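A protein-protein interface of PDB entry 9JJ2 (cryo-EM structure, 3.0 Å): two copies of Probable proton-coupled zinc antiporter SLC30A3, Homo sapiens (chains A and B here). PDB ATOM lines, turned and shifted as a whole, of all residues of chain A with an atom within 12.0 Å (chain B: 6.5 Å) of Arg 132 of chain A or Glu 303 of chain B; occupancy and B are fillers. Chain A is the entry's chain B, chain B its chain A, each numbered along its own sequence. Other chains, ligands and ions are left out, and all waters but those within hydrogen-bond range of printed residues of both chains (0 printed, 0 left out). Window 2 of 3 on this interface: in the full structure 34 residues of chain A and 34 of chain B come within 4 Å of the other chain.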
ATOM      1  N   ARG A 128      -0.673 -30.648  -4.515  1.00  0.00           N
ATOM      2  CA  ARG A 128      -0.073 -30.951  -5.807  1.00  0.00           C
ATOM      3  C   ARG A 128       1.404 -30.573  -5.795  1.00  0.00           C
ATOM      4  O   ARG A 128       1.748 -29.455  -5.397  1.00  0.00           O
ATOM      5  CB  ARG A 128      -0.802 -30.213  -6.923  1.00  0.00           C
ATOM      6  CG  ARG A 128      -2.104 -30.870  -7.345  1.00  0.00           C
ATOM      7  CD  ARG A 128      -2.830 -30.037  -8.385  1.00  0.00           C
ATOM      8  NE  ARG A 128      -2.407 -30.358  -9.742  1.00  0.00           N
ATOM      9  CZ  ARG A 128      -2.641 -29.594 -10.798  1.00  0.00           C
ATOM     10  NH1 ARG A 128      -3.288 -28.445 -10.691  1.00  0.00           N
ATOM     11  NH2 ARG A 128      -2.217 -29.992 -11.994  1.00  0.00           N
ATOM     12  N   PRO A 129       2.297 -31.464  -6.215  1.00  0.00           N
ATOM     13  CA  PRO A 129       3.727 -31.146  -6.187  1.00  0.00           C
ATOM     14  C   PRO A 129       4.088 -30.100  -7.228  1.00  0.00           C
ATOM     15  O   PRO A 129       3.395 -29.907  -8.229  1.00  0.00           O
ATOM     16  CB  PRO A 129       4.394 -32.489  -6.496  1.00  0.00           C
ATOM     17  CG  PRO A 129       3.381 -33.222  -7.302  1.00  0.00           C
ATOM     18  CD  PRO A 129       2.035 -32.798  -6.779  1.00  0.00           C
ATOM     19  N   ALA A 130       5.201 -29.417  -6.971  1.00  0.00           N
ATOM     20  CA  ALA A 130       5.691 -28.403  -7.893  1.00  0.00           C
ATOM     21  C   ALA A 130       6.142 -29.049  -9.196  1.00  0.00           C
ATOM     22  O   ALA A 130       6.870 -30.046  -9.188  1.00  0.00           O
ATOM     23  CB  ALA A 130       6.842 -27.627  -7.260  1.00  0.00           C
ATOM     24  N   THR A 131       5.711 -28.478 -10.315  1.00  0.00           N
ATOM     25  CA  THR A 131       6.039 -29.014 -11.627  1.00  0.00           C
ATOM     26  C   THR A 131       7.288 -28.321 -12.167  1.00  0.00           C
ATOM     27  O   THR A 131       7.921 -27.508 -11.490  1.00  0.00           O
ATOM     28  CB  THR A 131       4.854 -28.858 -12.577  1.00  0.00           C
ATOM     29  OG1 THR A 131       4.446 -27.485 -12.613  1.00  0.00           O
ATOM     30  CG2 THR A 131       3.688 -29.713 -12.117  1.00  0.00           C
ATOM     31  N   ARG A 132       7.659 -28.646 -13.403  1.00  0.00           N
ATOM     32  CA  ARG A 132       8.801 -28.017 -14.048  1.00  0.00           C
ATOM     33  C   ARG A 132       8.473 -26.642 -14.609  1.00  0.00           C
ATOM     34  O   ARG A 132       9.392 -25.924 -15.016  1.00  0.00           O
ATOM     35  CB  ARG A 132       9.334 -28.922 -15.157  1.00  0.00           C
ATOM     36  CG  ARG A 132       9.591 -30.344 -14.691  1.00  0.00           C
ATOM     37  CD  ARG A 132      10.250 -31.184 -15.765  1.00  0.00           C
ATOM     38  NE  ARG A 132      10.133 -30.574 -17.083  1.00  0.00           N
ATOM     39  CZ  ARG A 132      10.821 -30.964 -18.147  1.00  0.00           C
ATOM     40  NH1 ARG A 132      11.661 -31.983 -18.090  1.00  0.00           N
ATOM     41  NH2 ARG A 132      10.656 -30.319 -19.298  1.00  0.00           N
ATOM     42  N   THR A 133       7.197 -26.266 -14.653  1.00  0.00           N
ATOM     43  CA  THR A 133       6.795 -24.921 -15.031  1.00  0.00           C
ATOM     44  C   THR A 133       6.332 -24.083 -13.851  1.00  0.00           C
ATOM     45  O   THR A 133       6.059 -22.893 -14.029  1.00  0.00           O
ATOM     46  CB  THR A 133       5.675 -24.967 -16.082  1.00  0.00           C
ATOM     47  OG1 THR A 133       4.404 -25.020 -15.424  1.00  0.00           O
ATOM     48  CG2 THR A 133       5.829 -26.187 -16.971  1.00  0.00           C
ATOM     49  N   MET A 134       6.220 -24.671 -12.661  1.00  0.00           N
ATOM     50  CA  MET A 134       5.900 -23.952 -11.428  1.00  0.00           C
ATOM     51  C   MET A 134       6.896 -24.439 -10.381  1.00  0.00           C
ATOM     52  O   MET A 134       6.616 -25.383  -9.638  1.00  0.00           O
ATOM     53  CB  MET A 134       4.459 -24.189 -10.995  1.00  0.00           C
ATOM     54  CG  MET A 134       3.424 -23.579 -11.916  1.00  0.00           C
ATOM     55  SD  MET A 134       2.759 -22.040 -11.264  1.00  0.00           S
ATOM     56  CE  MET A 134       1.919 -21.399 -12.706  1.00  0.00           C
ATOM     57  N   THR A 135       8.056 -23.786 -10.324  1.00  0.00           N
ATOM     58  CA  THR A 135       9.145 -24.264  -9.482  1.00  0.00           C
ATOM     59  C   THR A 135       8.886 -24.038  -8.000  1.00  0.00           C
ATOM     60  O   THR A 135       9.537 -24.677  -7.168  1.00  0.00           O
ATOM     61  CB  THR A 135      10.448 -23.586  -9.888  1.00  0.00           C
ATOM     62  OG1 THR A 135      10.187 -22.215 -10.209  1.00  0.00           O
ATOM     63  CG2 THR A 135      11.044 -24.274 -11.101  1.00  0.00           C
ATOM     64  N   PHE A 136       7.963 -23.147  -7.651  1.00  0.00           N
ATOM     65  CA  PHE A 136       7.632 -22.879  -6.260  1.00  0.00           C
ATOM     66  C   PHE A 136       6.396 -23.625  -5.785  1.00  0.00           C
ATOM     67  O   PHE A 136       6.164 -23.698  -4.574  1.00  0.00           O
ATOM     68  CB  PHE A 136       7.422 -21.378  -6.047  1.00  0.00           C
ATOM     69  CG  PHE A 136       8.693 -20.615  -5.848  1.00  0.00           C
ATOM     70  CD1 PHE A 136       9.419 -20.746  -4.682  1.00  0.00           C
ATOM     71  CD2 PHE A 136       9.165 -19.769  -6.832  1.00  0.00           C
ATOM     72  CE1 PHE A 136      10.588 -20.047  -4.499  1.00  0.00           C
ATOM     73  CE2 PHE A 136      10.331 -19.069  -6.653  1.00  0.00           C
ATOM     74  CZ  PHE A 136      11.044 -19.208  -5.486  1.00  0.00           C
ATOM     75  N   GLY A 137       5.602 -24.174  -6.697  1.00  0.00           N
ATOM     76  CA  GLY A 137       4.370 -24.832  -6.322  1.00  0.00           C
ATOM     77  C   GLY A 137       3.162 -24.014  -6.717  1.00  0.00           C
ATOM     78  O   GLY A 137       3.196 -23.298  -7.721  1.00  0.00           O
ATOM     79  N   TRP A 138       2.092 -24.096  -5.930  1.00  0.00           N
ATOM     80  CA  TRP A 138       0.863 -23.371  -6.223  1.00  0.00           C
ATOM     81  C   TRP A 138       0.407 -22.556  -5.021  1.00  0.00           C
ATOM     82  O   TRP A 138      -0.793 -22.428  -4.772  1.00  0.00           O
ATOM     83  CB  TRP A 138      -0.240 -24.329  -6.666  1.00  0.00           C
ATOM     84  CG  TRP A 138       0.171 -25.251  -7.761  1.00  0.00           C
ATOM     85  CD1 TRP A 138       0.951 -26.362  -7.649  1.00  0.00           C
ATOM     86  CD2 TRP A 138      -0.184 -25.146  -9.140  1.00  0.00           C
ATOM     87  NE1 TRP A 138       1.108 -26.953  -8.878  1.00  0.00           N
ATOM     88  CE2 TRP A 138       0.420 -26.225  -9.810  1.00  0.00           C
ATOM     89  CE3 TRP A 138      -0.954 -24.242  -9.876  1.00  0.00           C
ATOM     90  CZ2 TRP A 138       0.278 -26.425 -11.178  1.00  0.00           C
ATOM     91  CZ3 TRP A 138      -1.093 -24.441 -11.231  1.00  0.00           C
ATOM     92  CH2 TRP A 138      -0.481 -25.523 -11.870  1.00  0.00           C
ATOM     93  N   THR B 296       7.779 -20.565 -14.322  1.00  0.00           N
ATOM     94  CA  THR B 296       8.944 -20.341 -15.158  1.00  0.00           C
ATOM     95  C   THR B 296       8.580 -19.401 -16.303  1.00  0.00           C
ATOM     96  O   THR B 296       7.503 -19.533 -16.894  1.00  0.00           O
ATOM     97  CB  THR B 296       9.460 -21.669 -15.712  1.00  0.00           C
ATOM     98  OG1 THR B 296       9.304 -22.689 -14.720  1.00  0.00           O
ATOM     99  CG2 THR B 296      10.924 -21.563 -16.082  1.00  0.00           C
ATOM    100  N   GLY B 301      13.496 -22.162 -20.432  1.00  0.00           N
ATOM    101  CA  GLY B 301      13.077 -23.527 -20.169  1.00  0.00           C
ATOM    102  C   GLY B 301      13.814 -24.100 -18.971  1.00  0.00           C
ATOM    103  O   GLY B 301      15.006 -23.857 -18.788  1.00  0.00           O
ATOM    104  N   PHE B 302      13.083 -24.861 -18.156  1.00  0.00           N
ATOM    105  CA  PHE B 302      13.680 -25.469 -16.971  1.00  0.00           C
ATOM    106  C   PHE B 302      14.785 -26.447 -17.345  1.00  0.00           C
ATOM    107  O   PHE B 302      15.865 -26.440 -16.739  1.00  0.00           O
ATOM    108  CB  PHE B 302      12.591 -26.170 -16.159  1.00  0.00           C
ATOM    109  CG  PHE B 302      13.072 -26.761 -14.867  1.00  0.00           C
ATOM    110  CD1 PHE B 302      13.071 -26.010 -13.707  1.00  0.00           C
ATOM    111  CD2 PHE B 302      13.503 -28.074 -14.807  1.00  0.00           C
ATOM    112  CE1 PHE B 302      13.502 -26.553 -12.518  1.00  0.00           C
ATOM    113  CE2 PHE B 302      13.936 -28.620 -13.620  1.00  0.00           C
ATOM    114  CZ  PHE B 302      13.935 -27.859 -12.474  1.00  0.00           C
ATOM    115  N   GLU B 303      14.534 -27.293 -18.340  1.00  0.00           N
ATOM    116  CA  GLU B 303      15.516 -28.306 -18.722  1.00  0.00           C
ATOM    117  C   GLU B 303      16.814 -27.709 -19.248  1.00  0.00           C
ATOM    118  O   GLU B 303      17.889 -28.169 -18.825  1.00  0.00           O
ATOM    119  CB  GLU B 303      14.893 -29.268 -19.736  1.00  0.00           C
ATOM    120  CG  GLU B 303      14.382 -30.549 -19.126  1.00  0.00           C
ATOM    121  CD  GLU B 303      15.335 -31.122 -18.104  1.00  0.00           C
ATOM    122  OE1 GLU B 303      16.498 -31.404 -18.460  1.00  0.00           O
ATOM    123  OE2 GLU B 303      14.918 -31.287 -16.940  1.00  0.00           O
ATOM    124  N   PRO B 304      16.808 -26.744 -20.180  1.00  0.00           N
ATOM    125  CA  PRO B 304      18.092 -26.168 -20.612  1.00  0.00           C
ATOM    126  C   PRO B 304      18.883 -25.552 -19.477  1.00  0.00           C
ATOM    127  O   PRO B 304      20.109 -25.698 -19.430  1.00  0.00           O
ATOM    128  CB  PRO B 304      17.671 -25.115 -21.646  1.00  0.00           C
ATOM    129  CG  PRO B 304      16.367 -25.586 -22.147  1.00  0.00           C
ATOM    130  CD  PRO B 304      15.688 -26.203 -20.969  1.00  0.00           C
ATOM    131  N   VAL B 305      18.207 -24.880 -18.544  1.00  0.00           N
ATOM    132  CA  VAL B 305      18.903 -24.286 -17.408  1.00  0.00           C
ATOM    133  C   VAL B 305      19.521 -25.368 -16.536  1.00  0.00           C
ATOM    134  O   VAL B 305      20.670 -25.245 -16.092  1.00  0.00           O
ATOM    135  CB  VAL B 305      17.950 -23.387 -16.605  1.00  0.00           C
ATOM    136  CG1 VAL B 305      18.650 -22.842 -15.383  1.00  0.00           C
ATOM    137  CG2 VAL B 305      17.454 -22.256 -17.467  1.00  0.00           C
ATOM    138  N   ARG B 306      18.776 -26.444 -16.275  1.00  0.00           N
ATOM    139  CA  ARG B 306      19.323 -27.522 -15.459  1.00  0.00           C
ATOM    140  C   ARG B 306      20.550 -28.137 -16.118  1.00  0.00           C
ATOM    141  O   ARG B 306      21.587 -28.320 -15.470  1.00  0.00           O
ATOM    142  CB  ARG B 306      18.259 -28.586 -15.199  1.00  0.00           C
ATOM    143  CG  ARG B 306      18.282 -29.118 -13.779  1.00  0.00           C
ATOM    144  CD  ARG B 306      17.884 -30.580 -13.713  1.00  0.00           C
ATOM    145  NE  ARG B 306      18.524 -31.366 -14.759  1.00  0.00           N
ATOM    146  CZ  ARG B 306      17.917 -32.311 -15.464  1.00  0.00           C
ATOM    147  NH1 ARG B 306      16.658 -32.642 -15.233  1.00  0.00           N
ATOM    148  NH2 ARG B 306      18.593 -32.945 -16.417  1.00  0.00           N
ATOM    149  N   ASP B 307      20.462 -28.438 -17.417  1.00  0.00           N
ATOM    150  CA  ASP B 307      21.612 -29.027 -18.098  1.00  0.00           C
ATOM    151  C   ASP B 307      22.798 -28.074 -18.106  1.00  0.00           C
ATOM    152  O   ASP B 307      23.944 -28.503 -17.938  1.00  0.00           O
ATOM    153  CB  ASP B 307      21.260 -29.452 -19.524  1.00  0.00           C
ATOM    154  CG  ASP B 307      19.873 -30.041 -19.636  1.00  0.00           C
ATOM    155  OD1 ASP B 307      19.193 -29.774 -20.649  1.00  0.00           O
ATOM    156  OD2 ASP B 307      19.463 -30.778 -18.716  1.00  0.00           O
ATOM    157  N   THR B 308      22.547 -26.775 -18.289  1.00  0.00           N
ATOM    158  CA  THR B 308      23.632 -25.804 -18.217  1.00  0.00           C
ATOM    159  C   THR B 308      24.298 -25.833 -16.851  1.00  0.00           C
ATOM    160  O   THR B 308      25.529 -25.771 -16.747  1.00  0.00           O
ATOM    161  CB  THR B 308      23.102 -24.405 -18.525  1.00  0.00           C
ATOM    162  OG1 THR B 308      22.721 -24.330 -19.904  1.00  0.00           O
ATOM    163  CG2 THR B 308      24.161 -23.355 -18.241  1.00  0.00           C
ATOM    164  N   LEU B 321      16.109 -25.917  -7.935  1.00  0.00           N
ATOM    165  CA  LEU B 321      16.250 -24.954  -9.018  1.00  0.00           C
ATOM    166  C   LEU B 321      14.955 -24.160  -9.120  1.00  0.00           C
ATOM    167  O   LEU B 321      13.910 -24.709  -9.478  1.00  0.00           O
ATOM    168  CB  LEU B 321      16.574 -25.667 -10.328  1.00  0.00           C
ATOM    169  CG  LEU B 321      16.725 -24.809 -11.580  1.00  0.00           C
ATOM    170  CD1 LEU B 321      17.788 -23.756 -11.380  1.00  0.00           C
ATOM    171  CD2 LEU B 321      17.069 -25.684 -12.765  1.00  0.00           C
ATOM    172  N   LEU B 323      13.087 -20.930 -10.867  1.00  0.00           N
ATOM    173  CA  LEU B 323      13.091 -19.957 -11.949  1.00  0.00           C
ATOM    174  C   LEU B 323      11.767 -19.215 -11.936  1.00  0.00           C
ATOM    175  O   LEU B 323      10.703 -19.840 -11.942  1.00  0.00           O
ATOM    176  CB  LEU B 323      13.309 -20.629 -13.306  1.00  0.00           C
ATOM    177  CG  LEU B 323      14.416 -21.679 -13.367  1.00  0.00           C
ATOM    178  CD1 LEU B 323      14.355 -22.439 -14.670  1.00  0.00           C
ATOM    179  CD2 LEU B 323      15.767 -21.026 -13.195  1.00  0.00           C
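The side-chain hydroxyl of Thr 296 of chain B sits at hydrogen-bond distance from the backbone carbonyl oxygen of Arg 132 of chain A. O of Thr 133 of chain A sits at hydrogen-bond distance from N of Thr 296 of chain B, 2.9 Å away. NH1 of Arg 132 of chain A lies within salt-bridge range of OE2 of Glu 303 of chain B, at 3.5 Å. The backbone carbonyl oxygen (O) of Leu 323 of chain B sits at hydrogen-bond distance from the side-chain hydroxyl (OG1) of Thr 135 of chain A.
The guanidinium group of Arg 306 of chain B lies within salt-bridge range of the side-chain carboxylate of Glu 303 of chain B (2.8 Å).
Phe 302 of chain B touches Arg 132 of chain A. CG2 of Thr 135 of chain A touches CE1 of Phe 302 of chain B, at 3.6 Å. Leu 321 of chain B touches Thr 135 of chain A.
Of the printed residues of chain B, Arg 132 of chain A touches Thr 296 (3.2 Å), Phe 302 (3.4 Å) and Glu 303 (3.2 Å). Of the printed residues of chain B, Thr 133 of chain A touches Thr 296. Printed residues of chain B within 4 Å of Thr 135 of chain A: Phe 302 (3.6 Å), Leu 321 (3.3 Å) and Leu 323 (3.0 Å). Of chain A, only Arg 132 and Thr 133 come within 4 Å of Thr 296 of chain B. Of chain A, only Arg 132 and Thr 135 come within 4 Å of Phe 302 of chain B. Printed residues of chain A within 4 Å of Glu 303 of chain B: Arg 132 (3.2 Å). No residue of chain A comes within 4 Å of Val 305 of chain B. No residue of chain A comes within 4 Å of Arg 306 of chain B. Of the printed residues of chain A, Leu 321 of chain B touches Thr 135. Of the printed residues of chain A, Leu 323 of chain B touches Thr 135 (3.0 Å). The nearest residue of chain B that does not touch Arg 132 of chain A is Arg 306 of chain B (5.8 Å). The nearest printed residue of chain A that does not touch Leu 321 of chain B is Phe 136 of chain A (6.4 Å).
Printed residues of chain A that touch a printed residue of chain B: Arg 132, Thr 133 and Thr 135. Along chain A the printed residues that touch a printed residue of chain B span positions 132 to 135. Of the 11 printed residues of chain B, 5 touch a printed residue of chain A. Among the printed residues, 7 pairs touch across the chains. Among the printed residues, Asp or Glu carboxylates within 4 Å of a Lys or Arg side-chain nitrogen of the other chain: Arg 132 of chain A with Glu 303 of chain B (3.5 Å).
No position is printed for both chains. Of the 7 pairs that touch across the chains among the printed residues, none has its exchanged pair printed and touching as well.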
